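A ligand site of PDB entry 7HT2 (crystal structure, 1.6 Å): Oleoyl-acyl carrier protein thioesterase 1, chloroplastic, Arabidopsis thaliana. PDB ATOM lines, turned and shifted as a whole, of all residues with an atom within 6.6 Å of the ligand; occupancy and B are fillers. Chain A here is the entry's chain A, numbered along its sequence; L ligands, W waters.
Water W4 bridges a nitrogen (N1) of the ligand (3.0 Å) and the backbone NH of Thr 70 (3.1 Å). Water W2 lies within hydrogen-bond range of the backbone NH of Glu 227 and the guanidinium group of Arg 131.
The backbone carbonyl oxygen (O) of Thr 70 lies within hydrogen-bond range of a nitrogen (N1) of the ligand (3.0 Å). A nitrogen (N2) of the ligand is in hydrogen-bond range of the backbone carbonyl oxygen of Arg 131, at 3.0 Å.
OG1 of Thr 70 lies within hydrogen-bond range of ND2 of Asn 196, 2.9 Å away. N of Tyr 224 is in hydrogen-bond range of O of Ala 71 (3.0 Å). O of Ile 276 sits at hydrogen-bond distance from N of Arg 225, at 2.9 Å. N of Arg 226 is in hydrogen-bond range of O of Ile 276 (3.1 Å). The backbone NH (N) of Val 69 sits at hydrogen-bond distance from the backbone carbonyl oxygen (O) of Val 124 (2.9 Å). The guanidinium group of Arg 131 lies within salt-bridge range of the side-chain carboxylate of Glu 227. The side-chain carboxylate (OE1) of Glu 227 is in hydrogen-bond range of a ring nitrogen (ND1) of His 193 (2.6 Å).
Merely in contact with the ligand: Tyr 224, Leu 133, Glu 227, Asn 196, Met 126, Arg 226, Arg 225 and Val 69. Ten residues have an atom within 4 Å of the ligand: Val 69, Thr 70, Met 126, Arg 131, Leu 133, Asn 196, Tyr 224, Arg 225, Arg 226 and Glu 227. The nearest printed residue that does not touch the ligand is Tyr 199 (4.2 Å).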
ATOM      1  N   VAL A  69      25.781   3.830 -15.796  1.00  0.00           N
ATOM      2  CA  VAL A  69      25.122   3.030 -14.756  1.00  0.00           C
ATOM      3  C   VAL A  69      23.696   2.693 -15.191  1.00  0.00           C
ATOM      4  O   VAL A  69      23.068   3.467 -15.925  1.00  0.00           O
ATOM      5  CB  VAL A  69      25.152   3.619 -13.334  1.00  0.00           C
ATOM      6  CG1 VAL A  69      26.594   3.891 -12.889  1.00  0.00           C
ATOM      7  CG2 VAL A  69      24.282   4.874 -13.235  1.00  0.00           C
ATOM      8  N   THR A  70      23.184   1.550 -14.733  1.00  0.00           N
ATOM      9  CA  THR A  70      21.845   1.109 -15.152  1.00  0.00           C
ATOM     10  C   THR A  70      20.732   1.895 -14.481  1.00  0.00           C
ATOM     11  O   THR A  70      20.733   2.056 -13.251  1.00  0.00           O
ATOM     12  CB  THR A  70      21.618  -0.402 -14.952  1.00  0.00           C
ATOM     13  OG1 THR A  70      22.851  -1.125 -15.139  1.00  0.00           O
ATOM     14  CG2 THR A  70      20.537  -0.951 -15.867  1.00  0.00           C
ATOM     15  N   ALA A  71      19.793   2.415 -15.275  1.00  0.00           N
ATOM     16  CA  ALA A  71      18.628   3.143 -14.757  1.00  0.00           C
ATOM     17  C   ALA A  71      17.398   2.209 -14.769  1.00  0.00           C
ATOM     18  O   ALA A  71      16.565   2.268 -13.871  1.00  0.00           O
ATOM     19  CB  ALA A  71      18.340   4.357 -15.613  1.00  0.00           C
ATOM     20  N   TRP A 123      20.611   3.294 -19.671  1.00  0.00           N
ATOM     21  CA  TRP A 123      21.831   3.614 -18.957  1.00  0.00           C
ATOM     22  C   TRP A 123      22.002   5.132 -18.945  1.00  0.00           C
ATOM     23  O   TRP A 123      21.683   5.797 -19.933  1.00  0.00           O
ATOM     24  CB  TRP A 123      23.044   2.931 -19.660  1.00  0.00           C
ATOM     25  CG  TRP A 123      22.943   1.432 -19.709  1.00  0.00           C
ATOM     26  CD1 TRP A 123      22.146   0.679 -20.522  1.00  0.00           C
ATOM     27  CD2 TRP A 123      23.682   0.509 -18.900  1.00  0.00           C
ATOM     28  NE1 TRP A 123      22.337  -0.662 -20.263  1.00  0.00           N
ATOM     29  CE2 TRP A 123      23.282  -0.796 -19.270  1.00  0.00           C
ATOM     30  CE3 TRP A 123      24.657   0.648 -17.890  1.00  0.00           C
ATOM     31  CZ2 TRP A 123      23.797  -1.944 -18.664  1.00  0.00           C
ATOM     32  CZ3 TRP A 123      25.193  -0.490 -17.319  1.00  0.00           C
ATOM     33  CH2 TRP A 123      24.770  -1.766 -17.706  1.00  0.00           C
ATOM     34  N   VAL A 124      22.442   5.669 -17.792  1.00  0.00           N
ATOM     35  CA  VAL A 124      22.686   7.100 -17.644  1.00  0.00           C
ATOM     36  C   VAL A 124      24.142   7.326 -17.250  1.00  0.00           C
ATOM     37  O   VAL A 124      24.798   6.434 -16.710  1.00  0.00           O
ATOM     38  CB  VAL A 124      21.711   7.774 -16.652  1.00  0.00           C
ATOM     39  CG1 VAL A 124      20.304   7.834 -17.228  1.00  0.00           C
ATOM     40  CG2 VAL A 124      21.718   7.060 -15.315  1.00  0.00           C
ATOM     41  N   MET A 126      27.279   8.814 -15.141  1.00  0.00           N
ATOM     42  CA  MET A 126      27.529   9.230 -13.763  1.00  0.00           C
ATOM     43  C   MET A 126      29.019   9.508 -13.569  1.00  0.00           C
ATOM     44  O   MET A 126      29.872   8.767 -14.068  1.00  0.00           O
ATOM     45  CB  MET A 126      27.123   8.090 -12.814  1.00  0.00           C
ATOM     46  CG  MET A 126      27.235   8.454 -11.333  1.00  0.00           C
ATOM     47  SD  MET A 126      26.918   7.062 -10.213  1.00  0.00           S
ATOM     48  CE  MET A 126      28.444   6.172 -10.369  1.00  0.00           C
ATOM     49  N   ARG A 131      29.480  10.569  -7.871  1.00  0.00           N
ATOM     50  CA  ARG A 131      28.239   9.818  -8.084  1.00  0.00           C
ATOM     51  C   ARG A 131      27.079  10.704  -8.592  1.00  0.00           C
ATOM     52  O   ARG A 131      25.921  10.297  -8.545  1.00  0.00           O
ATOM     53  CB  ARG A 131      27.844   8.975  -6.853  1.00  0.00           C
ATOM     54  CG  ARG A 131      28.952   8.025  -6.434  1.00  0.00           C
ATOM     55  CD  ARG A 131      28.541   7.046  -5.343  1.00  0.00           C
ATOM     56  NE  ARG A 131      27.428   6.175  -5.725  1.00  0.00           N
ATOM     57  CZ  ARG A 131      27.542   5.078  -6.475  1.00  0.00           C
ATOM     58  NH1 ARG A 131      28.722   4.728  -6.968  1.00  0.00           N
ATOM     59  NH2 ARG A 131      26.475   4.333  -6.750  1.00  0.00           N
ATOM     60  N   ARG A 132      27.392  11.883  -9.149  1.00  0.00           N
ATOM     61  CA  ARG A 132      26.418  12.804  -9.709  1.00  0.00           C
ATOM     62  C   ARG A 132      26.121  12.460 -11.164  1.00  0.00           C
ATOM     63  O   ARG A 132      27.047  12.204 -11.946  1.00  0.00           O
ATOM     64  CB  ARG A 132      26.898  14.252  -9.590  1.00  0.00           C
ATOM     65  CG  ARG A 132      27.115  14.647  -8.131  1.00  0.00           C
ATOM     66  CD  ARG A 132      27.561  16.089  -7.975  1.00  0.00           C
ATOM     67  NE  ARG A 132      26.608  17.051  -8.541  1.00  0.00           N
ATOM     68  CZ  ARG A 132      25.482  17.439  -7.934  1.00  0.00           C
ATOM     69  NH1 ARG A 132      25.148  16.924  -6.755  1.00  0.00           N
ATOM     70  NH2 ARG A 132      24.691  18.329  -8.510  1.00  0.00           N
ATOM     71  N   LEU A 133      24.815  12.382 -11.509  1.00  0.00           N
ATOM     72  CA  LEU A 133      24.397  12.066 -12.871  1.00  0.00           C
ATOM     73  C   LEU A 133      24.504  13.286 -13.780  1.00  0.00           C
ATOM     74  O   LEU A 133      24.470  14.429 -13.305  1.00  0.00           O
ATOM     75  CB  LEU A 133      22.937  11.583 -12.852  1.00  0.00           C
ATOM     76  CG  LEU A 133      22.683  10.337 -12.053  1.00  0.00           C
ATOM     77  CD1 LEU A 133      21.188  10.025 -12.005  1.00  0.00           C
ATOM     78  CD2 LEU A 133      23.492   9.163 -12.584  1.00  0.00           C
ATOM     79  N   HIS A 193      31.519  -4.333  -6.822  1.00  0.00           N
ATOM     80  CA  HIS A 193      30.181  -3.751  -6.757  1.00  0.00           C
ATOM     81  C   HIS A 193      29.179  -4.911  -6.794  1.00  0.00           C
ATOM     82  O   HIS A 193      29.419  -5.925  -7.452  1.00  0.00           O
ATOM     83  CB  HIS A 193      29.933  -2.845  -7.984  1.00  0.00           C
ATOM     84  CG  HIS A 193      30.724  -1.575  -7.949  1.00  0.00           C
ATOM     85  ND1 HIS A 193      30.117  -0.359  -7.675  1.00  0.00           N
ATOM     86  CD2 HIS A 193      32.060  -1.374  -8.091  1.00  0.00           C
ATOM     87  CE1 HIS A 193      31.101   0.538  -7.654  1.00  0.00           C
ATOM     88  NE2 HIS A 193      32.283  -0.021  -7.902  1.00  0.00           N
ATOM     89  N   VAL A 194      27.998  -4.746  -6.182  1.00  0.00           N
ATOM     90  CA  VAL A 194      26.954  -5.766  -6.261  1.00  0.00           C
ATOM     91  C   VAL A 194      26.486  -5.903  -7.728  1.00  0.00           C
ATOM     92  O   VAL A 194      26.204  -4.888  -8.380  1.00  0.00           O
ATOM     93  CB  VAL A 194      25.786  -5.453  -5.311  1.00  0.00           C
ATOM     94  CG1 VAL A 194      24.635  -6.446  -5.511  1.00  0.00           C
ATOM     95  CG2 VAL A 194      26.284  -5.460  -3.867  1.00  0.00           C
ATOM     96  N   ASN A 196      24.172  -6.317 -10.824  1.00  0.00           N
ATOM     97  CA  ASN A 196      22.749  -5.966 -11.039  1.00  0.00           C
ATOM     98  C   ASN A 196      21.799  -7.162 -10.994  1.00  0.00           C
ATOM     99  O   ASN A 196      20.628  -6.990 -10.629  1.00  0.00           O
ATOM    100  CB  ASN A 196      22.537  -5.270 -12.391  1.00  0.00           C
ATOM    101  CG  ASN A 196      23.153  -3.903 -12.482  1.00  0.00           C
ATOM    102  OD1 ASN A 196      23.328  -3.191 -11.485  1.00  0.00           O
ATOM    103  ND2 ASN A 196      23.502  -3.534 -13.718  1.00  0.00           N
ATOM    104  N   TYR A 199      19.910  -8.003  -7.702  1.00  0.00           N
ATOM    105  CA  TYR A 199      18.660  -7.302  -7.382  1.00  0.00           C
ATOM    106  C   TYR A 199      17.425  -8.035  -7.940  1.00  0.00           C
ATOM    107  O   TYR A 199      16.391  -8.070  -7.294  1.00  0.00           O
ATOM    108  CB  TYR A 199      18.667  -5.869  -7.901  1.00  0.00           C
ATOM    109  CG  TYR A 199      19.841  -5.048  -7.398  1.00  0.00           C
ATOM    110  CD1 TYR A 199      19.953  -4.707  -6.057  1.00  0.00           C
ATOM    111  CD2 TYR A 199      20.827  -4.619  -8.269  1.00  0.00           C
ATOM    112  CE1 TYR A 199      21.032  -3.946  -5.598  1.00  0.00           C
ATOM    113  CE2 TYR A 199      21.868  -3.811  -7.821  1.00  0.00           C
ATOM    114  CZ  TYR A 199      21.985  -3.497  -6.485  1.00  0.00           C
ATOM    115  OH  TYR A 199      23.038  -2.737  -6.041  1.00  0.00           O
ATOM    116  N   TYR A 224      16.192   1.102 -11.156  1.00  0.00           N
ATOM    117  CA  TYR A 224      17.328   1.209 -10.255  1.00  0.00           C
ATOM    118  C   TYR A 224      17.448   2.672  -9.707  1.00  0.00           C
ATOM    119  O   TYR A 224      17.550   3.644 -10.477  1.00  0.00           O
ATOM    120  CB  TYR A 224      18.617   0.736 -10.991  1.00  0.00           C
ATOM    121  CG  TYR A 224      18.584  -0.716 -11.445  1.00  0.00           C
ATOM    122  CD1 TYR A 224      18.156  -1.059 -12.717  1.00  0.00           C
ATOM    123  CD2 TYR A 224      19.052  -1.723 -10.626  1.00  0.00           C
ATOM    124  CE1 TYR A 224      18.145  -2.395 -13.146  1.00  0.00           C
ATOM    125  CE2 TYR A 224      18.994  -3.060 -11.016  1.00  0.00           C
ATOM    126  CZ  TYR A 224      18.556  -3.393 -12.279  1.00  0.00           C
ATOM    127  OH  TYR A 224      18.545  -4.721 -12.671  1.00  0.00           O
ATOM    128  N   ARG A 225      17.378   2.822  -8.372  1.00  0.00           N
ATOM    129  CA  ARG A 225      17.403   4.161  -7.761  1.00  0.00           C
ATOM    130  C   ARG A 225      18.679   4.431  -6.967  1.00  0.00           C
ATOM    131  O   ARG A 225      19.138   5.575  -6.883  1.00  0.00           O
ATOM    132  CB  ARG A 225      16.177   4.325  -6.845  1.00  0.00           C
ATOM    133  CG  ARG A 225      14.845   3.914  -7.489  1.00  0.00           C
ATOM    134  CD  ARG A 225      14.496   4.763  -8.700  1.00  0.00           C
ATOM    135  NE  ARG A 225      13.624   5.881  -8.350  1.00  0.00           N
ATOM    136  CZ  ARG A 225      12.387   6.049  -8.804  1.00  0.00           C
ATOM    137  NH1 ARG A 225      11.876   5.190  -9.685  1.00  0.00           N
ATOM    138  NH2 ARG A 225      11.662   7.087  -8.404  1.00  0.00           N
ATOM    139  N   ARG A 226      19.219   3.405  -6.329  1.00  0.00           N
ATOM    140  CA  ARG A 226      20.419   3.531  -5.506  1.00  0.00           C
ATOM    141  C   ARG A 226      21.138   2.195  -5.511  1.00  0.00           C
ATOM    142  O   ARG A 226      20.499   1.157  -5.477  1.00  0.00           O
ATOM    143  CB  ARG A 226      20.009   3.894  -4.061  1.00  0.00           C
ATOM    144  CG  ARG A 226      21.165   4.161  -3.103  1.00  0.00           C
ATOM    145  CD  ARG A 226      20.618   4.438  -1.714  1.00  0.00           C
ATOM    146  NE  ARG A 226      21.622   4.865  -0.732  1.00  0.00           N
ATOM    147  CZ  ARG A 226      21.863   6.132  -0.424  1.00  0.00           C
ATOM    148  NH1 ARG A 226      21.231   7.113  -1.062  1.00  0.00           N
ATOM    149  NH2 ARG A 226      22.776   6.442   0.481  1.00  0.00           N
ATOM    150  N   GLU A 227      22.464   2.237  -5.451  1.00  0.00           N
ATOM    151  CA  GLU A 227      23.315   1.061  -5.410  1.00  0.00           C
ATOM    152  C   GLU A 227      23.447   0.477  -3.996  1.00  0.00           C
ATOM    153  O   GLU A 227      23.629   1.228  -3.040  1.00  0.00           O
ATOM    154  CB  GLU A 227      24.690   1.441  -5.953  1.00  0.00           C
ATOM    155  CG  GLU A 227      25.662   0.284  -6.048  1.00  0.00           C
ATOM    156  CD  GLU A 227      26.818   0.494  -6.997  1.00  0.00           C
ATOM    157  OE1 GLU A 227      27.604  -0.468  -7.176  1.00  0.00           O
ATOM    158  OE2 GLU A 227      26.948   1.596  -7.581  1.00  0.00           O
ATOM    159  N   CYS A 228      23.313  -0.853  -3.853  1.00  0.00           N
ATOM    160  CA  CYS A 228      23.460  -1.554  -2.567  1.00  0.00           C
ATOM    161  C   CYS A 228      24.971  -1.790  -2.344  1.00  0.00           C
ATOM    162  O   CYS A 228      25.684  -2.234  -3.254  1.00  0.00           O
ATOM    163  CB  CYS A 228      22.675  -2.868  -2.564  1.00  0.00           C
ATOM    164  SG  CYS A 228      22.970  -3.944  -1.135  1.00  0.00           S
ATOM    165  N   ILE A 276      16.106   1.228  -2.780  1.00  0.00           N
ATOM    166  CA  ILE A 276      17.222   0.885  -3.661  1.00  0.00           C
ATOM    167  C   ILE A 276      16.693   0.550  -5.069  1.00  0.00           C
ATOM    168  O   ILE A 276      17.272   1.011  -6.051  1.00  0.00           O
ATOM    169  CB  ILE A 276      18.234  -0.126  -3.091  1.00  0.00           C
ATOM    170  CG1 ILE A 276      17.646  -1.460  -2.885  1.00  0.00           C
ATOM    171  CG2 ILE A 276      18.953   0.362  -1.778  1.00  0.00           C
ATOM    172  CD1 ILE A 276      18.612  -2.456  -3.399  1.00  0.00           C
ATOM    173  N   ASN A 277      15.531  -0.128  -5.171  1.00  0.00           N
ATOM    174  CA  ASN A 277      14.922  -0.508  -6.451  1.00  0.00           C
ATOM    175  C   ASN A 277      13.410  -0.585  -6.312  1.00  0.00           C
ATOM    176  O   ASN A 277      12.910  -0.903  -5.241  1.00  0.00           O
ATOM    177  CB  ASN A 277      15.292  -2.018  -6.810  1.00  0.00           C
ATOM    178  CG  ASN A 277      16.618  -2.211  -7.452  1.00  0.00           C
ATOM    179  OD1 ASN A 277      17.601  -2.454  -6.800  1.00  0.00           O
ATOM    180  ND2 ASN A 277      16.659  -2.130  -8.760  1.00  0.00           N
HETATM  181  C1  LIG L   1      22.987   2.180  -9.431  1.00  0.00           C
HETATM  182  C2  LIG L   1      21.955   2.997  -8.991  1.00  0.00           C
HETATM  183  C3  LIG L   1      22.237   4.312  -8.631  1.00  0.00           C
HETATM  184  C4  LIG L   1      23.520   4.826  -8.741  1.00  0.00           C
HETATM  185  C5  LIG L   1      24.527   3.985  -9.189  1.00  0.00           C
HETATM  186  C6  LIG L   1      24.264   2.681  -9.554  1.00  0.00           C
HETATM  187  S1  LIG L   1      22.645   0.500  -9.851  1.00  0.00           S
HETATM  188  O1  LIG L   1      23.820  -0.266  -9.570  1.00  0.00           O
HETATM  189  O2  LIG L   1      21.420   0.152  -9.192  1.00  0.00           O
HETATM  190  N1  LIG L   1      22.402   0.433 -11.437  1.00  0.00           N
HETATM  191  C7  LIG L   1      23.828   6.238  -8.325  1.00  0.00           C
HETATM  192  C8  LIG L   1      23.442   7.252  -9.368  1.00  0.00           C
HETATM  193  N2  LIG L   1      23.483   8.611  -8.843  1.00  0.00           N
HETATM  194  C9  LIG L   1      22.361   9.298  -8.601  1.00  0.00           C
HETATM  195  C10 LIG L   1      22.539  10.706  -8.133  1.00  0.00           C
HETATM  196  O3  LIG L   1      21.249   8.808  -8.761  1.00  0.00           O
HETATM  197  O   HOH W   1      19.344  -0.578  -7.524  1.00  0.00           O
HETATM  198  O   HOH W   2      23.863   4.896  -5.214  1.00  0.00           O
HETATM  199  O   HOH W   3      25.066  -2.613  -7.867  1.00  0.00           O
HETATM  200  O   HOH W   4      25.088   0.042 -12.778  1.00  0.00           O
